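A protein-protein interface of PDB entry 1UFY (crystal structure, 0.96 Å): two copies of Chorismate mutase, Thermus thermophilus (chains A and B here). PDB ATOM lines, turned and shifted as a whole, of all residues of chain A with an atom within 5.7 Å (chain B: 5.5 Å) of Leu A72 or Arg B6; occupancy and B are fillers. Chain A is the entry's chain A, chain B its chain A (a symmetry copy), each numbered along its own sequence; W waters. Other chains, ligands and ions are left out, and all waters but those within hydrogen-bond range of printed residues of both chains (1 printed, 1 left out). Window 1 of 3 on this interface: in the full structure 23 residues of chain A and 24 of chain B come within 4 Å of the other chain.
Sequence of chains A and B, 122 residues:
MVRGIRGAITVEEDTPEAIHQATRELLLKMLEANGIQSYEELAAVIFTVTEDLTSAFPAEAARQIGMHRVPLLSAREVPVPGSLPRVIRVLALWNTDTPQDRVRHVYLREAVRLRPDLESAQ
Hydrophobic or aromatic side chains of chain B within 4 Å of the printed part of chain A: Leu B91.
Hydrophobic or aromatic side chains of chain A that line the printed part of chain B: Ile A46, Pro A71 and Leu A73.
Along chain A the printed residues that touch a printed residue of chain B span positions 46 to 73.
Among the printed residues, 6 pairs touch across the chains.
Among the printed residues, no Asp or Glu carboxylate lies within 4 Å of a Lys or Arg side-chain nitrogen of the other chain.
Among the printed residues, pairs that only touch across the chains: Ile A46 with Leu B91, Pro A71 with Gly B4, Pro A71 with Arg B6, Pro A71 with Leu B91 and Leu A73 with Leu B91.
No position is printed for both chains.
Of the 6 pairs that touch across the chains among the printed residues, none has its exchanged pair printed and touching as well.
The guanidinium group (NH1) of Arg B6 sits at hydrogen-bond distance from the backbone carbonyl oxygen (O) of Leu A72 (2.8 Å).
Water W1 bridges the backbone carbonyl oxygen of Leu A72 (3.2 Å) and the guanidinium group of Arg B6 (3.5 Å).
Of the printed residues of chain B, Ile A46 touches Leu B91 (3.995 Å).
Of the printed residues of chain B, Pro A71 touches Gly B4, Arg B6 and Leu B91.
Of chain B, only Arg B6 comes within 4 Å of Leu A72.
Of the printed residues of chain B, Leu A73 touches Leu B91 (3.9 Å).
Printed residues of chain A within 4 Å of Gly B4: Pro A71 (3.2 Å).
Of the printed residues of chain A, Arg B6 touches Pro A71 and Leu A72.
Ala B8 touches none of the printed residues of chain A.
Of the printed residues of chain A, Leu B91 touches Ile A46 (3.995 Å), Pro A71 (3.7 Å) and Leu A73 (3.9 Å).
N of Val B106 sits at hydrogen-bond distance from O of Arg B6, 3.0 Å away.
The backbone NH of Phe A47 sits at hydrogen-bond distance from the backbone carbonyl oxygen of Leu A73, at 2.8 Å.
The backbone NH (N) of Arg B6 lies within hydrogen-bond range of a ring nitrogen (ND1) of His B105, at 2.9 Å.
N of Val A45 lies within hydrogen-bond range of O of Pro A71, at 2.9 Å.
O of Val A45 sits at hydrogen-bond distance from N of Leu A73 (3.1 Å).
NE of Arg B6 is in hydrogen-bond range of O of Val B90, 2.9 Å away.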
ATOM      1  N   ALA A  44      21.670  14.674 -21.514  1.00  0.00           N
ATOM      2  CA  ALA A  44      20.944  15.550 -22.429  1.00  0.00           C
ATOM      3  C   ALA A  44      21.906  15.874 -23.572  1.00  0.00           C
ATOM      4  O   ALA A  44      23.123  15.710 -23.448  1.00  0.00           O
ATOM      5  CB  ALA A  44      20.524  16.847 -21.781  1.00  0.00           C
ATOM      6  N   VAL A  45      21.345  16.357 -24.674  1.00  0.00           N
ATOM      7  CA  VAL A  45      22.148  16.881 -25.797  1.00  0.00           C
ATOM      8  C   VAL A  45      21.540  18.207 -26.236  1.00  0.00           C
ATOM      9  O   VAL A  45      20.334  18.305 -26.468  1.00  0.00           O
ATOM     10  CB  VAL A  45      22.218  15.894 -26.968  1.00  0.00           C
ATOM     11  CG1 VAL A  45      23.097  16.468 -28.071  1.00  0.00           C
ATOM     12  CG2 VAL A  45      22.706  14.517 -26.537  1.00  0.00           C
ATOM     13  N   ILE A  46      22.410  19.220 -26.362  1.00  0.00           N
ATOM     14  CA  ILE A  46      22.027  20.542 -26.803  1.00  0.00           C
ATOM     15  C   ILE A  46      22.682  20.818 -28.155  1.00  0.00           C
ATOM     16  O   ILE A  46      23.858  20.530 -28.344  1.00  0.00           O
ATOM     17  CB  ILE A  46      22.398  21.612 -25.763  1.00  0.00           C
ATOM     18  CG1 ILE A  46      21.800  21.239 -24.385  1.00  0.00           C
ATOM     19  CG2 ILE A  46      21.972  22.998 -26.253  1.00  0.00           C
ATOM     20  CD1 ILE A  46      22.353  22.089 -23.245  1.00  0.00           C
ATOM     21  N   PHE A  47      21.933  21.359 -29.075  1.00  0.00           N
ATOM     22  CA  PHE A  47      22.402  21.701 -30.408  1.00  0.00           C
ATOM     23  C   PHE A  47      22.339  23.207 -30.625  1.00  0.00           C
ATOM     24  O   PHE A  47      21.381  23.858 -30.137  1.00  0.00           O
ATOM     25  CB  PHE A  47      21.506  21.065 -31.474  1.00  0.00           C
ATOM     26  CG  PHE A  47      21.372  19.573 -31.392  1.00  0.00           C
ATOM     27  CD1 PHE A  47      20.410  18.975 -30.635  1.00  0.00           C
ATOM     28  CD2 PHE A  47      22.225  18.742 -32.083  1.00  0.00           C
ATOM     29  CE1 PHE A  47      20.290  17.613 -30.548  1.00  0.00           C
ATOM     30  CE2 PHE A  47      22.127  17.373 -32.001  1.00  0.00           C
ATOM     31  CZ  PHE A  47      21.143  16.815 -31.242  1.00  0.00           C
ATOM     32  N   ALA A  59      17.286  17.990 -33.651  1.00  0.00           N
ATOM     33  CA  ALA A  59      16.712  16.950 -32.786  1.00  0.00           C
ATOM     34  C   ALA A  59      15.937  15.918 -33.576  1.00  0.00           C
ATOM     35  O   ALA A  59      15.846  14.768 -33.180  1.00  0.00           O
ATOM     36  CB  ALA A  59      15.826  17.604 -31.747  1.00  0.00           C
ATOM     37  N   GLU A  60      15.349  16.317 -34.720  1.00  0.00           N
ATOM     38  CA  GLU A  60      14.650  15.343 -35.569  1.00  0.00           C
ATOM     39  C   GLU A  60      15.639  14.300 -36.094  1.00  0.00           C
ATOM     40  O   GLU A  60      15.321  13.130 -36.161  1.00  0.00           O
ATOM     41  CB  GLU A  60      13.959  16.024 -36.735  1.00  0.00           C
ATOM     42  CG  GLU A  60      13.389  15.095 -37.790  1.00  0.00           C
ATOM     43  N   ALA A  62      18.445  13.445 -34.577  1.00  0.00           N
ATOM     44  CA  ALA A  62      18.784  12.615 -33.454  1.00  0.00           C
ATOM     45  C   ALA A  62      17.734  11.533 -33.225  1.00  0.00           C
ATOM     46  O   ALA A  62      18.067  10.388 -32.879  1.00  0.00           O
ATOM     47  CB  ALA A  62      18.973  13.486 -32.214  1.00  0.00           C
ATOM     48  N   ARG A  63      16.460  11.871 -33.434  1.00  0.00           N
ATOM     49  CA  ARG A  63      15.388  10.862 -33.327  1.00  0.00           C
ATOM     50  C   ARG A  63      15.422   9.863 -34.479  1.00  0.00           C
ATOM     51  O   ARG A  63      14.966   8.718 -34.267  1.00  0.00           O
ATOM     52  CB  ARG A  63      14.036  11.532 -33.113  1.00  0.00           C
ATOM     53  CG  ARG A  63      13.909  12.018 -31.677  1.00  0.00           C
ATOM     54  CD  ARG A  63      12.536  12.507 -31.295  1.00  0.00           C
ATOM     55  NE  ARG A  63      12.288  13.758 -31.932  1.00  0.00           N
ATOM     56  CZ  ARG A  63      12.629  14.950 -31.405  1.00  0.00           C
ATOM     57  NH1 ARG A  63      13.256  15.058 -30.221  1.00  0.00           N
ATOM     58  NH2 ARG A  63      12.354  16.068 -32.010  1.00  0.00           N
ATOM     59  N   MET A  67      17.117   8.704 -30.616  1.00  0.00           N
ATOM     60  CA  MET A  67      17.302   9.461 -29.389  1.00  0.00           C
ATOM     61  C   MET A  67      16.010   9.975 -28.782  1.00  0.00           C
ATOM     62  O   MET A  67      16.042  10.962 -28.025  1.00  0.00           O
ATOM     63  CB  MET A  67      18.343  10.566 -29.560  1.00  0.00           C
ATOM     64  CG  MET A  67      19.741  10.015 -29.788  1.00  0.00           C
ATOM     65  SD  MET A  67      20.992  11.257 -29.562  1.00  0.00           S
ATOM     66  CE  MET A  67      22.438  10.214 -29.800  1.00  0.00           C
ATOM     67  N   VAL A  70      16.474  10.422 -25.059  1.00  0.00           N
ATOM     68  CA  VAL A  70      17.501  11.384 -24.667  1.00  0.00           C
ATOM     69  C   VAL A  70      16.879  12.771 -24.739  1.00  0.00           C
ATOM     70  O   VAL A  70      16.323  13.146 -25.775  1.00  0.00           O
ATOM     71  CB  VAL A  70      18.730  11.315 -25.597  1.00  0.00           C
ATOM     72  CG1 VAL A  70      19.797  12.282 -25.137  1.00  0.00           C
ATOM     73  CG2 VAL A  70      19.277   9.909 -25.698  1.00  0.00           C
ATOM     74  N   PRO A  71      16.966  13.575 -23.687  1.00  0.00           N
ATOM     75  CA  PRO A  71      16.397  14.925 -23.738  1.00  0.00           C
ATOM     76  C   PRO A  71      17.251  15.834 -24.639  1.00  0.00           C
ATOM     77  O   PRO A  71      18.465  15.910 -24.440  1.00  0.00           O
ATOM     78  CB  PRO A  71      16.467  15.375 -22.283  1.00  0.00           C
ATOM     79  CG  PRO A  71      16.967  14.308 -21.489  1.00  0.00           C
ATOM     80  CD  PRO A  71      17.424  13.202 -22.336  1.00  0.00           C
ATOM     81  N   LEU A  72      16.607  16.492 -25.596  1.00  0.00           N
ATOM     82  CA  LEU A  72      17.274  17.274 -26.616  1.00  0.00           C
ATOM     83  C   LEU A  72      16.774  18.697 -26.611  1.00  0.00           C
ATOM     84  O   LEU A  72      15.579  18.945 -26.395  1.00  0.00           O
ATOM     85  CB  LEU A  72      17.001  16.671 -28.006  1.00  0.00           C
ATOM     86  CG  LEU A  72      17.297  15.197 -28.156  1.00  0.00           C
ATOM     87  CD1 LEU A  72      16.866  14.714 -29.513  1.00  0.00           C
ATOM     88  CD2 LEU A  72      18.723  14.836 -27.894  1.00  0.00           C
ATOM     89  N   LEU A  73      17.631  19.651 -26.922  1.00  0.00           N
ATOM     90  CA  LEU A  73      17.228  21.052 -27.026  1.00  0.00           C
ATOM     91  C   LEU A  73      18.062  21.745 -28.114  1.00  0.00           C
ATOM     92  O   LEU A  73      19.227  21.402 -28.237  1.00  0.00           O
ATOM     93  CB  LEU A  73      17.406  21.752 -25.693  1.00  0.00           C
ATOM     94  CG  LEU A  73      16.676  23.076 -25.496  1.00  0.00           C
ATOM     95  CD1 LEU A  73      15.182  22.888 -25.341  1.00  0.00           C
ATOM     96  CD2 LEU A  73      17.242  23.791 -24.297  1.00  0.00           C
ATOM     97  N   SER A  74      17.500  22.668 -28.854  1.00  0.00           N
ATOM     98  CA  SER A  74      18.227  23.365 -29.877  1.00  0.00           C
ATOM     99  C   SER A  74      18.048  24.878 -29.789  1.00  0.00           C
ATOM    100  O   SER A  74      17.032  25.385 -29.293  1.00  0.00           O
ATOM    101  CB  SER A  74      17.934  22.914 -31.316  1.00  0.00           C
ATOM    102  OG  SER A  74      16.619  22.919 -31.617  1.00  0.00           O
ATOM    103  N   GLY B   4      18.269  14.948 -17.912  1.00  0.00           N
ATOM    104  CA  GLY B   4      17.441  16.006 -18.419  1.00  0.00           C
ATOM    105  C   GLY B   4      15.970  15.655 -18.382  1.00  0.00           C
ATOM    106  O   GLY B   4      15.586  14.504 -18.595  1.00  0.00           O
ATOM    107  N   ILE B   5      15.145  16.667 -18.185  1.00  0.00           N
ATOM    108  CA  ILE B   5      13.704  16.553 -18.291  1.00  0.00           C
ATOM    109  C   ILE B   5      13.268  17.558 -19.339  1.00  0.00           C
ATOM    110  O   ILE B   5      13.596  18.766 -19.211  1.00  0.00           O
ATOM    111  CB  ILE B   5      12.959  16.838 -16.986  1.00  0.00           C
ATOM    112  CG1 ILE B   5      13.572  16.174 -15.779  1.00  0.00           C
ATOM    113  CG2 ILE B   5      11.484  16.498 -17.178  1.00  0.00           C
ATOM    114  CD1 ILE B   5      12.983  16.642 -14.458  1.00  0.00           C
ATOM    115  N   ARG B   6      12.572  17.120 -20.389  1.00  0.00           N
ATOM    116  CA  ARG B   6      12.043  18.013 -21.364  1.00  0.00           C
ATOM    117  C   ARG B   6      10.579  18.350 -21.094  1.00  0.00           C
ATOM    118  O   ARG B   6       9.788  17.494 -20.705  1.00  0.00           O
ATOM    119  CB  ARG B   6      12.155  17.441 -22.798  1.00  0.00           C
ATOM    120  CG  ARG B   6      13.474  17.740 -23.466  1.00  0.00           C
ATOM    121  CD  ARG B   6      13.803  19.257 -23.671  1.00  0.00           C
ATOM    122  NE  ARG B   6      12.711  19.987 -24.123  1.00  0.00           N
ATOM    123  CZ  ARG B   6      12.191  19.956 -25.332  1.00  0.00           C
ATOM    124  NH1 ARG B   6      12.825  19.379 -26.302  1.00  0.00           N
ATOM    125  NH2 ARG B   6      11.036  20.583 -25.555  1.00  0.00           N
ATOM    126  N   GLY B   7      10.255  19.603 -21.373  1.00  0.00           N
ATOM    127  CA  GLY B   7       8.903  20.060 -21.417  1.00  0.00           C
ATOM    128  C   GLY B   7       8.659  20.971 -22.610  1.00  0.00           C
ATOM    129  O   GLY B   7       9.615  21.568 -23.157  1.00  0.00           O
ATOM    130  N   ALA B   8       7.406  21.136 -22.994  1.00  0.00           N
ATOM    131  CA  ALA B   8       7.045  22.135 -23.958  1.00  0.00           C
ATOM    132  C   ALA B   8       5.571  22.516 -23.755  1.00  0.00           C
ATOM    133  O   ALA B   8       4.762  21.660 -23.335  1.00  0.00           O
ATOM    134  CB  ALA B   8       7.252  21.665 -25.378  1.00  0.00           C
ATOM    135  N   MET B  30       6.175  19.479 -14.779  1.00  0.00           N
ATOM    136  CA  MET B  30       7.406  18.703 -14.948  1.00  0.00           C
ATOM    137  C   MET B  30       7.906  18.167 -13.618  1.00  0.00           C
ATOM    138  O   MET B  30       8.350  17.016 -13.486  1.00  0.00           O
ATOM    139  CB  MET B  30       8.474  19.564 -15.592  1.00  0.00           C
ATOM    140  CG  MET B  30       8.197  19.867 -17.053  1.00  0.00           C
ATOM    141  SD  MET B  30       9.342  21.079 -17.757  1.00  0.00           S
ATOM    142  CE  MET B  30      10.836  20.078 -17.814  1.00  0.00           C
ATOM    143  N   ARG B  89       9.897  25.923 -24.637  1.00  0.00           N
ATOM    144  CA  ARG B  89      10.540  24.644 -24.370  1.00  0.00           C
ATOM    145  C   ARG B  89      11.403  24.761 -23.113  1.00  0.00           C
ATOM    146  O   ARG B  89      12.031  25.807 -22.882  1.00  0.00           O
ATOM    147  CB  ARG B  89      11.364  24.150 -25.524  1.00  0.00           C
ATOM    148  CG  ARG B  89      10.553  23.818 -26.759  1.00  0.00           C
ATOM    149  CD  ARG B  89      11.417  23.488 -27.961  1.00  0.00           C
ATOM    150  NE  ARG B  89      10.703  22.906 -29.085  1.00  0.00           N
ATOM    151  CZ  ARG B  89      10.109  23.582 -30.063  1.00  0.00           C
ATOM    152  NH1 ARG B  89      10.024  24.885 -30.078  1.00  0.00           N
ATOM    153  NH2 ARG B  89       9.544  22.890 -31.065  1.00  0.00           N
ATOM    154  N   VAL B  90      11.435  23.687 -22.347  1.00  0.00           N
ATOM    155  CA  VAL B  90      12.197  23.626 -21.122  1.00  0.00           C
ATOM    156  C   VAL B  90      13.104  22.391 -21.163  1.00  0.00           C
ATOM    157  O   VAL B  90      12.623  21.288 -21.484  1.00  0.00           O
ATOM    158  CB  VAL B  90      11.292  23.537 -19.882  1.00  0.00           C
ATOM    159  CG1 VAL B  90      12.108  23.502 -18.622  1.00  0.00           C
ATOM    160  CG2 VAL B  90      10.338  24.692 -19.835  1.00  0.00           C
ATOM    161  N   LEU B  91      14.366  22.546 -20.752  1.00  0.00           N
ATOM    162  CA  LEU B  91      15.287  21.440 -20.411  1.00  0.00           C
ATOM    163  C   LEU B  91      15.739  21.620 -18.959  1.00  0.00           C
ATOM    164  O   LEU B  91      16.565  22.496 -18.675  1.00  0.00           O
ATOM    165  CB  LEU B  91      16.487  21.390 -21.322  1.00  0.00           C
ATOM    166  CG  LEU B  91      17.522  20.324 -21.012  1.00  0.00           C
ATOM    167  CD1 LEU B  91      16.973  18.916 -21.195  1.00  0.00           C
ATOM    168  CD2 LEU B  91      18.745  20.486 -21.923  1.00  0.00           C
ATOM    169  N   ALA B  92      15.177  20.858 -18.039  1.00  0.00           N
ATOM    170  CA  ALA B  92      15.600  20.875 -16.654  1.00  0.00           C
ATOM    171  C   ALA B  92      16.698  19.850 -16.456  1.00  0.00           C
ATOM    172  O   ALA B  92      16.552  18.700 -16.920  1.00  0.00           O
ATOM    173  CB  ALA B  92      14.450  20.559 -15.734  1.00  0.00           C
ATOM    174  N   ARG B 104      10.021  11.415 -16.895  1.00  0.00           N
ATOM    175  CA  ARG B 104       8.772  11.750 -17.556  1.00  0.00           C
ATOM    176  C   ARG B 104       8.860  13.138 -18.174  1.00  0.00           C
ATOM    177  O   ARG B 104       9.063  14.135 -17.483  1.00  0.00           O
ATOM    178  CB  ARG B 104       7.613  11.682 -16.561  1.00  0.00           C
ATOM    179  CG  ARG B 104       7.486  10.248 -15.966  1.00  0.00           C
ATOM    180  CD  ARG B 104       6.907   9.294 -17.033  1.00  0.00           C
ATOM    181  NE  ARG B 104       7.121   7.915 -16.591  1.00  0.00           N
ATOM    182  CZ  ARG B 104       7.953   7.051 -17.190  1.00  0.00           C
ATOM    183  NH1 ARG B 104       8.715   7.317 -18.344  1.00  0.00           N
ATOM    184  NH2 ARG B 104       8.001   5.860 -16.550  1.00  0.00           N
ATOM    185  N   HIS B 105       8.699  13.197 -19.482  1.00  0.00           N
ATOM    186  CA  HIS B 105       8.768  14.412 -20.253  1.00  0.00           C
ATOM    187  C   HIS B 105       7.326  14.934 -20.461  1.00  0.00           C
ATOM    188  O   HIS B 105       6.411  14.142 -20.630  1.00  0.00           O
ATOM    189  CB  HIS B 105       9.522  14.179 -21.556  1.00  0.00           C
ATOM    190  CG  HIS B 105      10.862  13.581 -21.283  1.00  0.00           C
ATOM    191  ND1 HIS B 105      11.910  14.306 -20.724  1.00  0.00           N
ATOM    192  CD2 HIS B 105      11.269  12.275 -21.379  1.00  0.00           C
ATOM    193  CE1 HIS B 105      12.894  13.452 -20.543  1.00  0.00           C
ATOM    194  NE2 HIS B 105      12.551  12.220 -20.941  1.00  0.00           N
ATOM    195  N   VAL B 106       7.125  16.237 -20.446  1.00  0.00           N
ATOM    196  CA  VAL B 106       5.785  16.838 -20.359  1.00  0.00           C
ATOM    197  C   VAL B 106       5.540  17.809 -21.483  1.00  0.00           C
ATOM    198  O   VAL B 106       6.164  18.866 -21.566  1.00  0.00           O
ATOM    199  CB  VAL B 106       5.615  17.507 -18.987  1.00  0.00           C
ATOM    200  CG1 VAL B 106       4.199  18.138 -18.912  1.00  0.00           C
ATOM    201  CG2 VAL B 106       5.813  16.523 -17.860  1.00  0.00           C
ATOM    202  N   TYR B 107       4.579  17.476 -22.355  1.00  0.00           N
ATOM    203  CA  TYR B 107       4.233  18.257 -23.526  1.00  0.00           C
ATOM    204  C   TYR B 107       2.764  18.640 -23.428  1.00  0.00           C
ATOM    205  O   TYR B 107       1.907  17.736 -23.407  1.00  0.00           O
ATOM    206  CB  TYR B 107       4.561  17.481 -24.839  1.00  0.00           C
ATOM    207  CG  TYR B 107       6.046  17.420 -25.116  1.00  0.00           C
ATOM    208  CD1 TYR B 107       6.628  18.136 -26.123  1.00  0.00           C
ATOM    209  CD2 TYR B 107       6.903  16.661 -24.340  1.00  0.00           C
ATOM    210  CE1 TYR B 107       7.993  18.110 -26.369  1.00  0.00           C
ATOM    211  CE2 TYR B 107       8.254  16.619 -24.535  1.00  0.00           C
ATOM    212  CZ  TYR B 107       8.811  17.359 -25.554  1.00  0.00           C
ATOM    213  OH  TYR B 107      10.157  17.287 -25.751  1.00  0.00           O
HETATM  214  O   HOH W   1      14.511  19.818 -29.312  1.00  0.00           O
